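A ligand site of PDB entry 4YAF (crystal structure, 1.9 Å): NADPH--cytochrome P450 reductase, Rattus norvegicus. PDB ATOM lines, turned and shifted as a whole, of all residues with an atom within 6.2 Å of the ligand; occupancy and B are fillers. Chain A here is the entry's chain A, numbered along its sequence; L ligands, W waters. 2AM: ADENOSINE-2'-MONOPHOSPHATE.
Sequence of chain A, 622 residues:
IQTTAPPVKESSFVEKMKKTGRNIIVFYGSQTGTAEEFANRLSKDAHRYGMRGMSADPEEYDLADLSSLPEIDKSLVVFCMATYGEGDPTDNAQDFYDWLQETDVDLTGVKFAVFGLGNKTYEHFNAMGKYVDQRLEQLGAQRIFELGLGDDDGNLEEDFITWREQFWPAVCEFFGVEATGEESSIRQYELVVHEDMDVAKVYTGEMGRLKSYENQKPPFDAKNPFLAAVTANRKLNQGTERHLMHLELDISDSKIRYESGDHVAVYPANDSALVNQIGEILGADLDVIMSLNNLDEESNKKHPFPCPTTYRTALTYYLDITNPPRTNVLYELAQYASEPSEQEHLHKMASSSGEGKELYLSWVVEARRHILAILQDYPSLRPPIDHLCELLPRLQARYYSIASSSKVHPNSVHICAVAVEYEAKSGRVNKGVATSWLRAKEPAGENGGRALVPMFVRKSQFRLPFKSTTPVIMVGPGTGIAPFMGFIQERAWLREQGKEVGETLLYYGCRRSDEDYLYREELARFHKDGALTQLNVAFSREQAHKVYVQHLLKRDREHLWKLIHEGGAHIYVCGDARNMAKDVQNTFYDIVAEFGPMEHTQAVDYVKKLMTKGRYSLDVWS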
ATOM      1  N   ARG A 242      30.688 -10.918  36.383  1.00  0.00           N
ATOM      2  CA  ARG A 242      30.365  -9.525  36.655  1.00  0.00           C
ATOM      3  C   ARG A 242      30.201  -9.338  38.162  1.00  0.00           C
ATOM      4  O   ARG A 242      30.372 -10.278  38.946  1.00  0.00           O
ATOM      5  CB  ARG A 242      29.045  -9.177  35.961  1.00  0.00           C
ATOM      6  CG  ARG A 242      28.990  -9.638  34.517  1.00  0.00           C
ATOM      7  CD  ARG A 242      27.561 -10.026  34.130  1.00  0.00           C
ATOM      8  NE  ARG A 242      26.718  -8.866  33.891  1.00  0.00           N
ATOM      9  CZ  ARG A 242      25.386  -8.891  33.875  1.00  0.00           C
ATOM     10  NH1 ARG A 242      24.743 -10.035  34.097  1.00  0.00           N
ATOM     11  NH2 ARG A 242      24.708  -7.789  33.625  1.00  0.00           N
ATOM     12  N   PRO A 477      13.998  -9.391  33.788  1.00  0.00           N
ATOM     13  CA  PRO A 477      15.259 -10.156  33.738  1.00  0.00           C
ATOM     14  C   PRO A 477      16.461  -9.303  34.174  1.00  0.00           C
ATOM     15  O   PRO A 477      16.454  -8.072  34.054  1.00  0.00           O
ATOM     16  CB  PRO A 477      15.330 -10.582  32.276  1.00  0.00           C
ATOM     17  CG  PRO A 477      14.607  -9.472  31.551  1.00  0.00           C
ATOM     18  CD  PRO A 477      13.419  -9.213  32.453  1.00  0.00           C
ATOM     19  N   GLY A 478      17.483  -9.968  34.704  1.00  0.00           N
ATOM     20  CA  GLY A 478      18.676  -9.272  35.158  1.00  0.00           C
ATOM     21  C   GLY A 478      18.382  -8.277  36.270  1.00  0.00           C
ATOM     22  O   GLY A 478      17.615  -8.579  37.190  1.00  0.00           O
ATOM     23  N   THR A 479      18.960  -7.081  36.183  1.00  0.00           N
ATOM     24  CA  THR A 479      18.723  -6.065  37.213  1.00  0.00           C
ATOM     25  C   THR A 479      17.285  -5.553  37.155  1.00  0.00           C
ATOM     26  O   THR A 479      16.868  -4.751  37.980  1.00  0.00           O
ATOM     27  CB  THR A 479      19.699  -4.860  37.085  1.00  0.00           C
ATOM     28  OG1 THR A 479      19.641  -4.323  35.757  1.00  0.00           O
ATOM     29  CG2 THR A 479      21.118  -5.288  37.417  1.00  0.00           C
ATOM     30  N   GLY A 509      14.912 -13.658  34.642  1.00  0.00           N
ATOM     31  CA  GLY A 509      15.867 -14.305  33.762  1.00  0.00           C
ATOM     32  C   GLY A 509      17.296 -13.897  34.088  1.00  0.00           C
ATOM     33  O   GLY A 509      17.540 -12.782  34.512  1.00  0.00           O
ATOM     34  N   CYS A 510      18.213 -14.827  33.884  1.00  0.00           N
ATOM     35  CA  CYS A 510      19.633 -14.594  34.112  1.00  0.00           C
ATOM     36  C   CYS A 510      20.377 -15.566  33.219  1.00  0.00           C
ATOM     37  O   CYS A 510      19.763 -16.367  32.515  1.00  0.00           O
ATOM     38  CB  CYS A 510      19.984 -14.806  35.588  1.00  0.00           C
ATOM     39  SG  CYS A 510      19.689 -16.485  36.211  1.00  0.00           S
ATOM     40  N   ARG A 511      21.711 -15.504  33.228  1.00  0.00           N
ATOM     41  CA  ARG A 511      22.523 -16.395  32.398  1.00  0.00           C
ATOM     42  C   ARG A 511      22.524 -17.852  32.867  1.00  0.00           C
ATOM     43  O   ARG A 511      22.188 -18.763  32.107  1.00  0.00           O
ATOM     44  CB  ARG A 511      23.966 -15.867  32.340  1.00  0.00           C
ATOM     45  CG  ARG A 511      24.083 -14.460  31.777  1.00  0.00           C
ATOM     46  CD  ARG A 511      25.534 -13.991  31.747  1.00  0.00           C
ATOM     47  NE  ARG A 511      25.636 -12.629  31.249  1.00  0.00           N
ATOM     48  CZ  ARG A 511      26.786 -11.971  31.098  1.00  0.00           C
ATOM     49  NH1 ARG A 511      27.933 -12.557  31.418  1.00  0.00           N
ATOM     50  NH2 ARG A 511      26.789 -10.735  30.621  1.00  0.00           N
ATOM     51  N   ASP A 516      24.497 -15.792  38.047  1.00  0.00           N
ATOM     52  CA  ASP A 516      23.910 -14.519  38.430  1.00  0.00           C
ATOM     53  C   ASP A 516      22.397 -14.541  38.662  1.00  0.00           C
ATOM     54  O   ASP A 516      21.674 -13.649  38.205  1.00  0.00           O
ATOM     55  CB  ASP A 516      24.253 -13.470  37.374  1.00  0.00           C
ATOM     56  CG  ASP A 516      23.897 -13.910  35.961  1.00  0.00           C
ATOM     57  OD1 ASP A 516      23.267 -14.986  35.834  1.00  0.00           O
ATOM     58  OD2 ASP A 516      24.231 -13.193  35.002  1.00  0.00           O
ATOM     59  N   ALA A 538      14.068 -17.876  33.266  1.00  0.00           N
ATOM     60  CA  ALA A 538      14.693 -18.235  32.006  1.00  0.00           C
ATOM     61  C   ALA A 538      16.202 -18.144  32.165  1.00  0.00           C
ATOM     62  O   ALA A 538      16.740 -17.065  32.412  1.00  0.00           O
ATOM     63  CB  ALA A 538      14.216 -17.294  30.901  1.00  0.00           C
ATOM     64  N   PHE A 539      16.883 -19.279  32.042  1.00  0.00           N
ATOM     65  CA  PHE A 539      18.341 -19.303  32.138  1.00  0.00           C
ATOM     66  C   PHE A 539      18.816 -19.258  30.678  1.00  0.00           C
ATOM     67  O   PHE A 539      18.785 -20.257  29.971  1.00  0.00           O
ATOM     68  CB  PHE A 539      18.799 -20.574  32.835  1.00  0.00           C
ATOM     69  CG  PHE A 539      18.335 -20.670  34.265  1.00  0.00           C
ATOM     70  CD1 PHE A 539      18.794 -19.768  35.222  1.00  0.00           C
ATOM     71  CD2 PHE A 539      17.399 -21.623  34.648  1.00  0.00           C
ATOM     72  CE1 PHE A 539      18.329 -19.815  36.535  1.00  0.00           C
ATOM     73  CE2 PHE A 539      16.928 -21.685  35.967  1.00  0.00           C
ATOM     74  CZ  PHE A 539      17.393 -20.776  36.913  1.00  0.00           C
ATOM     75  N   SER A 540      19.244 -18.071  30.252  1.00  0.00           N
ATOM     76  CA  SER A 540      19.648 -17.846  28.874  1.00  0.00           C
ATOM     77  C   SER A 540      20.854 -18.604  28.352  1.00  0.00           C
ATOM     78  O   SER A 540      20.920 -18.872  27.150  1.00  0.00           O
ATOM     79  CB  SER A 540      19.866 -16.346  28.639  1.00  0.00           C
ATOM     80  OG  SER A 540      20.971 -15.870  29.384  1.00  0.00           O
ATOM     81  N   ARG A 541      21.784 -18.954  29.229  1.00  0.00           N
ATOM     82  CA  ARG A 541      23.006 -19.631  28.812  1.00  0.00           C
ATOM     83  C   ARG A 541      23.206 -21.062  29.326  1.00  0.00           C
ATOM     84  O   ARG A 541      24.301 -21.602  29.204  1.00  0.00           O
ATOM     85  CB  ARG A 541      24.212 -18.772  29.190  1.00  0.00           C
ATOM     86  CG  ARG A 541      24.079 -17.336  28.690  1.00  0.00           C
ATOM     87  CD  ARG A 541      25.343 -16.506  28.889  1.00  0.00           C
ATOM     88  NE  ARG A 541      25.126 -15.147  28.382  1.00  0.00           N
ATOM     89  CZ  ARG A 541      26.077 -14.238  28.279  1.00  0.00           C
ATOM     90  NH1 ARG A 541      27.321 -14.519  28.646  1.00  0.00           N
ATOM     91  NH2 ARG A 541      25.780 -13.033  27.806  1.00  0.00           N
ATOM     92  N   LYS A 546      19.071 -19.725  23.302  1.00  0.00           N
ATOM     93  CA  LYS A 546      18.693 -18.741  24.299  1.00  0.00           C
ATOM     94  C   LYS A 546      17.292 -19.018  24.834  1.00  0.00           C
ATOM     95  O   LYS A 546      16.403 -19.409  24.086  1.00  0.00           O
ATOM     96  CB  LYS A 546      18.687 -17.329  23.679  1.00  0.00           C
ATOM     97  CG  LYS A 546      20.041 -16.809  23.238  1.00  0.00           C
ATOM     98  CD  LYS A 546      21.003 -16.678  24.405  1.00  0.00           C
ATOM     99  CE  LYS A 546      22.249 -15.891  24.010  1.00  0.00           C
ATOM    100  NZ  LYS A 546      23.219 -15.808  25.139  1.00  0.00           N
ATOM    101  N   VAL A 547      17.126 -18.861  26.136  1.00  0.00           N
ATOM    102  CA  VAL A 547      15.807 -18.995  26.748  1.00  0.00           C
ATOM    103  C   VAL A 547      15.647 -17.671  27.467  1.00  0.00           C
ATOM    104  O   VAL A 547      16.417 -17.364  28.371  1.00  0.00           O
ATOM    105  CB  VAL A 547      15.714 -20.150  27.761  1.00  0.00           C
ATOM    106  CG1 VAL A 547      14.300 -20.174  28.370  1.00  0.00           C
ATOM    107  CG2 VAL A 547      16.000 -21.469  27.079  1.00  0.00           C
ATOM    108  N   TYR A 548      14.670 -16.880  27.020  1.00  0.00           N
ATOM    109  CA  TYR A 548      14.407 -15.572  27.592  1.00  0.00           C
ATOM    110  C   TYR A 548      13.026 -15.505  28.223  1.00  0.00           C
ATOM    111  O   TYR A 548      12.180 -16.358  27.959  1.00  0.00           O
ATOM    112  CB  TYR A 548      14.505 -14.487  26.518  1.00  0.00           C
ATOM    113  CG  TYR A 548      15.874 -14.281  25.901  1.00  0.00           C
ATOM    114  CD1 TYR A 548      17.036 -14.407  26.661  1.00  0.00           C
ATOM    115  CD2 TYR A 548      15.995 -13.873  24.570  1.00  0.00           C
ATOM    116  CE1 TYR A 548      18.295 -14.117  26.116  1.00  0.00           C
ATOM    117  CE2 TYR A 548      17.241 -13.580  24.019  1.00  0.00           C
ATOM    118  CZ  TYR A 548      18.387 -13.696  24.803  1.00  0.00           C
ATOM    119  OH  TYR A 548      19.607 -13.371  24.254  1.00  0.00           O
ATOM    120  N   VAL A 549      12.768 -14.475  29.008  1.00  0.00           N
ATOM    121  CA  VAL A 549      11.474 -14.335  29.654  1.00  0.00           C
ATOM    122  C   VAL A 549      10.291 -14.390  28.679  1.00  0.00           C
ATOM    123  O   VAL A 549       9.259 -14.989  28.982  1.00  0.00           O
ATOM    124  CB  VAL A 549      11.403 -13.045  30.511  1.00  0.00           C
ATOM    125  CG1 VAL A 549      12.294 -13.178  31.750  1.00  0.00           C
ATOM    126  CG2 VAL A 549      11.829 -11.837  29.694  1.00  0.00           C
ATOM    127  N   GLN A 550      10.419 -13.769  27.501  1.00  0.00           N
ATOM    128  CA  GLN A 550       9.311 -13.781  26.555  1.00  0.00           C
ATOM    129  C   GLN A 550       8.982 -15.190  26.062  1.00  0.00           C
ATOM    130  O   GLN A 550       7.854 -15.453  25.624  1.00  0.00           O
ATOM    131  CB  GLN A 550       9.591 -12.870  25.347  1.00  0.00           C
ATOM    132  CG  GLN A 550      10.865 -13.192  24.594  1.00  0.00           C
ATOM    133  CD  GLN A 550      12.042 -12.363  25.074  1.00  0.00           C
ATOM    134  OE1 GLN A 550      12.169 -12.081  26.257  1.00  0.00           O
ATOM    135  NE2 GLN A 550      12.909 -11.976  24.147  1.00  0.00           N
ATOM    136  N   ASP A 576      16.190  -3.824  30.671  1.00  0.00           N
ATOM    137  CA  ASP A 576      16.693  -3.367  29.373  1.00  0.00           C
ATOM    138  C   ASP A 576      15.610  -2.827  28.449  1.00  0.00           C
ATOM    139  O   ASP A 576      14.698  -3.551  28.039  1.00  0.00           O
ATOM    140  CB  ASP A 576      17.427  -4.506  28.671  1.00  0.00           C
ATOM    141  CG  ASP A 576      17.910  -4.114  27.301  1.00  0.00           C
ATOM    142  OD1 ASP A 576      18.763  -3.208  27.223  1.00  0.00           O
ATOM    143  OD2 ASP A 576      17.428  -4.706  26.309  1.00  0.00           O
ATOM    144  N   ASN A 579      16.204  -3.813  23.842  1.00  0.00           N
ATOM    145  CA  ASN A 579      15.754  -5.032  23.195  1.00  0.00           C
ATOM    146  C   ASN A 579      14.702  -5.844  23.953  1.00  0.00           C
ATOM    147  O   ASN A 579      13.672  -6.201  23.395  1.00  0.00           O
ATOM    148  CB  ASN A 579      16.958  -5.929  22.874  1.00  0.00           C
ATOM    149  CG  ASN A 579      17.918  -5.297  21.871  1.00  0.00           C
ATOM    150  OD1 ASN A 579      18.826  -4.555  22.244  1.00  0.00           O
ATOM    151  ND2 ASN A 579      17.690  -5.579  20.595  1.00  0.00           N
ATOM    152  N   MET A 580      14.960  -6.110  25.223  1.00  0.00           N
ATOM    153  CA  MET A 580      14.044  -6.896  26.026  1.00  0.00           C
ATOM    154  C   MET A 580      12.617  -6.336  26.071  1.00  0.00           C
ATOM    155  O   MET A 580      11.660  -7.033  25.739  1.00  0.00           O
ATOM    156  CB  MET A 580      14.613  -7.070  27.438  1.00  0.00           C
ATOM    157  CG  MET A 580      13.783  -7.972  28.362  1.00  0.00           C
ATOM    158  SD  MET A 580      12.387  -7.112  29.092  1.00  0.00           S
ATOM    159  CE  MET A 580      13.276  -6.107  30.352  1.00  0.00           C
ATOM    160  N   ALA A 581      12.470  -5.072  26.471  1.00  0.00           N
ATOM    161  CA  ALA A 581      11.149  -4.459  26.550  1.00  0.00           C
ATOM    162  C   ALA A 581      10.344  -4.619  25.249  1.00  0.00           C
ATOM    163  O   ALA A 581       9.165  -4.956  25.278  1.00  0.00           O
ATOM    164  CB  ALA A 581      11.266  -2.981  26.898  1.00  0.00           C
ATOM    165  N   ASP A 583      10.881  -6.862  22.773  1.00  0.00           N
ATOM    166  CA  ASP A 583      10.592  -8.266  22.492  1.00  0.00           C
ATOM    167  C   ASP A 583       9.421  -8.724  23.345  1.00  0.00           C
ATOM    168  O   ASP A 583       8.561  -9.473  22.878  1.00  0.00           O
ATOM    169  CB  ASP A 583      11.815  -9.146  22.753  1.00  0.00           C
ATOM    170  CG  ASP A 583      12.907  -8.950  21.726  1.00  0.00           C
ATOM    171  OD1 ASP A 583      12.588  -8.557  20.579  1.00  0.00           O
ATOM    172  OD2 ASP A 583      14.091  -9.190  22.054  1.00  0.00           O
ATOM    173  N   VAL A 584       9.382  -8.281  24.601  1.00  0.00           N
ATOM    174  CA  VAL A 584       8.304  -8.666  25.491  1.00  0.00           C
ATOM    175  C   VAL A 584       6.996  -8.051  24.998  1.00  0.00           C
ATOM    176  O   VAL A 584       5.948  -8.718  24.953  1.00  0.00           O
ATOM    177  CB  VAL A 584       8.593  -8.203  26.942  1.00  0.00           C
ATOM    178  CG1 VAL A 584       7.354  -8.327  27.799  1.00  0.00           C
ATOM    179  CG2 VAL A 584       9.716  -9.069  27.520  1.00  0.00           C
HETATM  180  P   2AM L   1      22.003 -13.175  27.372  1.00  0.00           P
HETATM  181  O1P 2AM L   1      21.553 -12.837  25.998  1.00  0.00           O
HETATM  182  O2P 2AM L   1      22.862 -12.150  28.002  1.00  0.00           O
HETATM  183  O3P 2AM L   1      22.489 -14.564  27.514  1.00  0.00           O
HETATM  184  C5' 2AM L   1      19.982 -10.304  31.878  1.00  0.00           C
HETATM  185  O5' 2AM L   1      20.870  -9.620  30.987  1.00  0.00           O
HETATM  186  C4' 2AM L   1      19.255 -11.412  31.109  1.00  0.00           C
HETATM  187  O4' 2AM L   1      18.527 -10.857  29.998  1.00  0.00           O
HETATM  188  C3' 2AM L   1      20.270 -12.390  30.524  1.00  0.00           C
HETATM  189  O3' 2AM L   1      19.812 -13.738  30.714  1.00  0.00           O
HETATM  190  C2' 2AM L   1      20.251 -12.032  29.043  1.00  0.00           C
HETATM  191  O2' 2AM L   1      20.650 -13.164  28.247  1.00  0.00           O
HETATM  192  C1' 2AM L   1      18.783 -11.721  28.871  1.00  0.00           C
HETATM  193  N9  2AM L   1      18.462 -11.057  27.589  1.00  0.00           N
HETATM  194  C8  2AM L   1      19.309 -10.530  26.717  1.00  0.00           C
HETATM  195  N7  2AM L   1      18.610 -10.028  25.710  1.00  0.00           N
HETATM  196  C5  2AM L   1      17.317 -10.247  25.962  1.00  0.00           C
HETATM  197  C6  2AM L   1      16.227  -9.974  25.248  1.00  0.00           C
HETATM  198  N6  2AM L   1      16.409  -9.504  24.020  1.00  0.00           N
HETATM  199  N1  2AM L   1      15.004 -10.304  25.676  1.00  0.00           N
HETATM  200  C2  2AM L   1      14.867 -10.965  26.908  1.00  0.00           C
HETATM  201  N3  2AM L   1      16.033 -11.231  27.633  1.00  0.00           N
HETATM  202  C4  2AM L   1      17.227 -10.871  27.124  1.00  0.00           C
HETATM  203  O   HOH W   1      20.227  -8.021  24.276  1.00  0.00           O
HETATM  204  O   HOH W   2      23.157  -9.768  26.716  1.00  0.00           O
HETATM  205  O   HOH W   3      15.197 -12.952  29.707  1.00  0.00           O
HETATM  206  O   HOH W   4      23.509 -10.916  30.203  1.00  0.00           O
HETATM  207  O   HOH W   5      17.157 -14.788  30.505  1.00  0.00           O
HETATM  208  O   HOH W   6      23.428 -11.969  24.363  1.00  0.00           O
HETATM  209  O   HOH W   7      17.415  -8.257  29.594  1.00  0.00           O
HETATM  210  O   HOH W   8      21.912 -12.111  33.969  1.00  0.00           O
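Pro 477 touches the ligand (CB to O4', 3.9 Å). Gly 478 touches the ligand (CA to C5', 3.7 Å). Arg 511 touches the ligand. Asn 579 touches the ligand (CB to N6, 3.8 Å). Met 580 touches the ligand (CG to C2, 3.5 Å). Hydrophobic or aromatic side chains that line the ligand: Pro 477, Tyr 548 and Met 580. Within 4 Å of the ligand: Pro 477, Gly 478, Cys 510, Arg 511, Ser 540, Arg 541, Lys 546, Tyr 548, Gln 550, Asn 579, Met 580 and Asp 583. The nearest printed residue that does not touch the ligand is Gly 509 (4.05 Å).
The side-chain hydroxyl (OG) of Ser 540 lies within hydrogen-bond range of an oxygen (O3P) of the ligand, 2.7 Å away. O of Cys 510 lies close to O3' of the ligand, at 3.2 Å. The side-chain hydroxyl (OH) of Tyr 548 lies within hydrogen-bond range of an oxygen (O1P) of the ligand (2.7 Å). The side-chain carboxylate of Asp 583 sits at hydrogen-bond distance from a nitrogen (N6) of the ligand (3.1 Å). The guanidinium group (NE) of Arg 541 lies within salt-bridge range of an oxygen (O3P) of the ligand, 2.8 Å away. NZ of Lys 546 is in salt-bridge range of O3P of the ligand. The side-chain amide nitrogen (NE2) of Gln 550 lies within hydrogen-bond range of a nitrogen (N1) of the ligand (3.1 Å).
Water W4 lies within hydrogen-bond range of an oxygen (O2P) of the ligand (2.6 Å) and the guanidinium group of Arg 511 (2.9 Å). Water W3 lies within hydrogen-bond range of N3 of the ligand (2.8 Å) and N of Val 549 (3.0 Å). Water W5 lies within hydrogen-bond range of O3' of the ligand, O of Ala 538 and O of Val 547. Water W8 bridges OD2 of Asp 516 and N of Arg 511.
N of Ser 540 sits close to O of Val 547, 3.5 Å away. The backbone carbonyl oxygen of Arg 511 sits at hydrogen-bond distance from the backbone NH of Arg 541, at 2.9 Å. The backbone NH of Gly 478 is in hydrogen-bond range of the backbone carbonyl oxygen of Gly 509 (2.8 Å). The backbone carbonyl oxygen (O) of Ala 538 lies within hydrogen-bond range of the backbone NH (N) of Cys 510 (3.1 Å). The backbone NH (N) of Asn 579 lies within hydrogen-bond range of the side-chain carboxylate (OD2) of Asp 576 (2.9 Å). The backbone NH of Arg 511 is in hydrogen-bond range of the side-chain carboxylate of Asp 516, 3.1 Å away. N of Met 580 is in hydrogen-bond range of OD2 of Asp 576, 3.0 Å away. O of Cys 510 lies within hydrogen-bond range of N of Ser 540.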
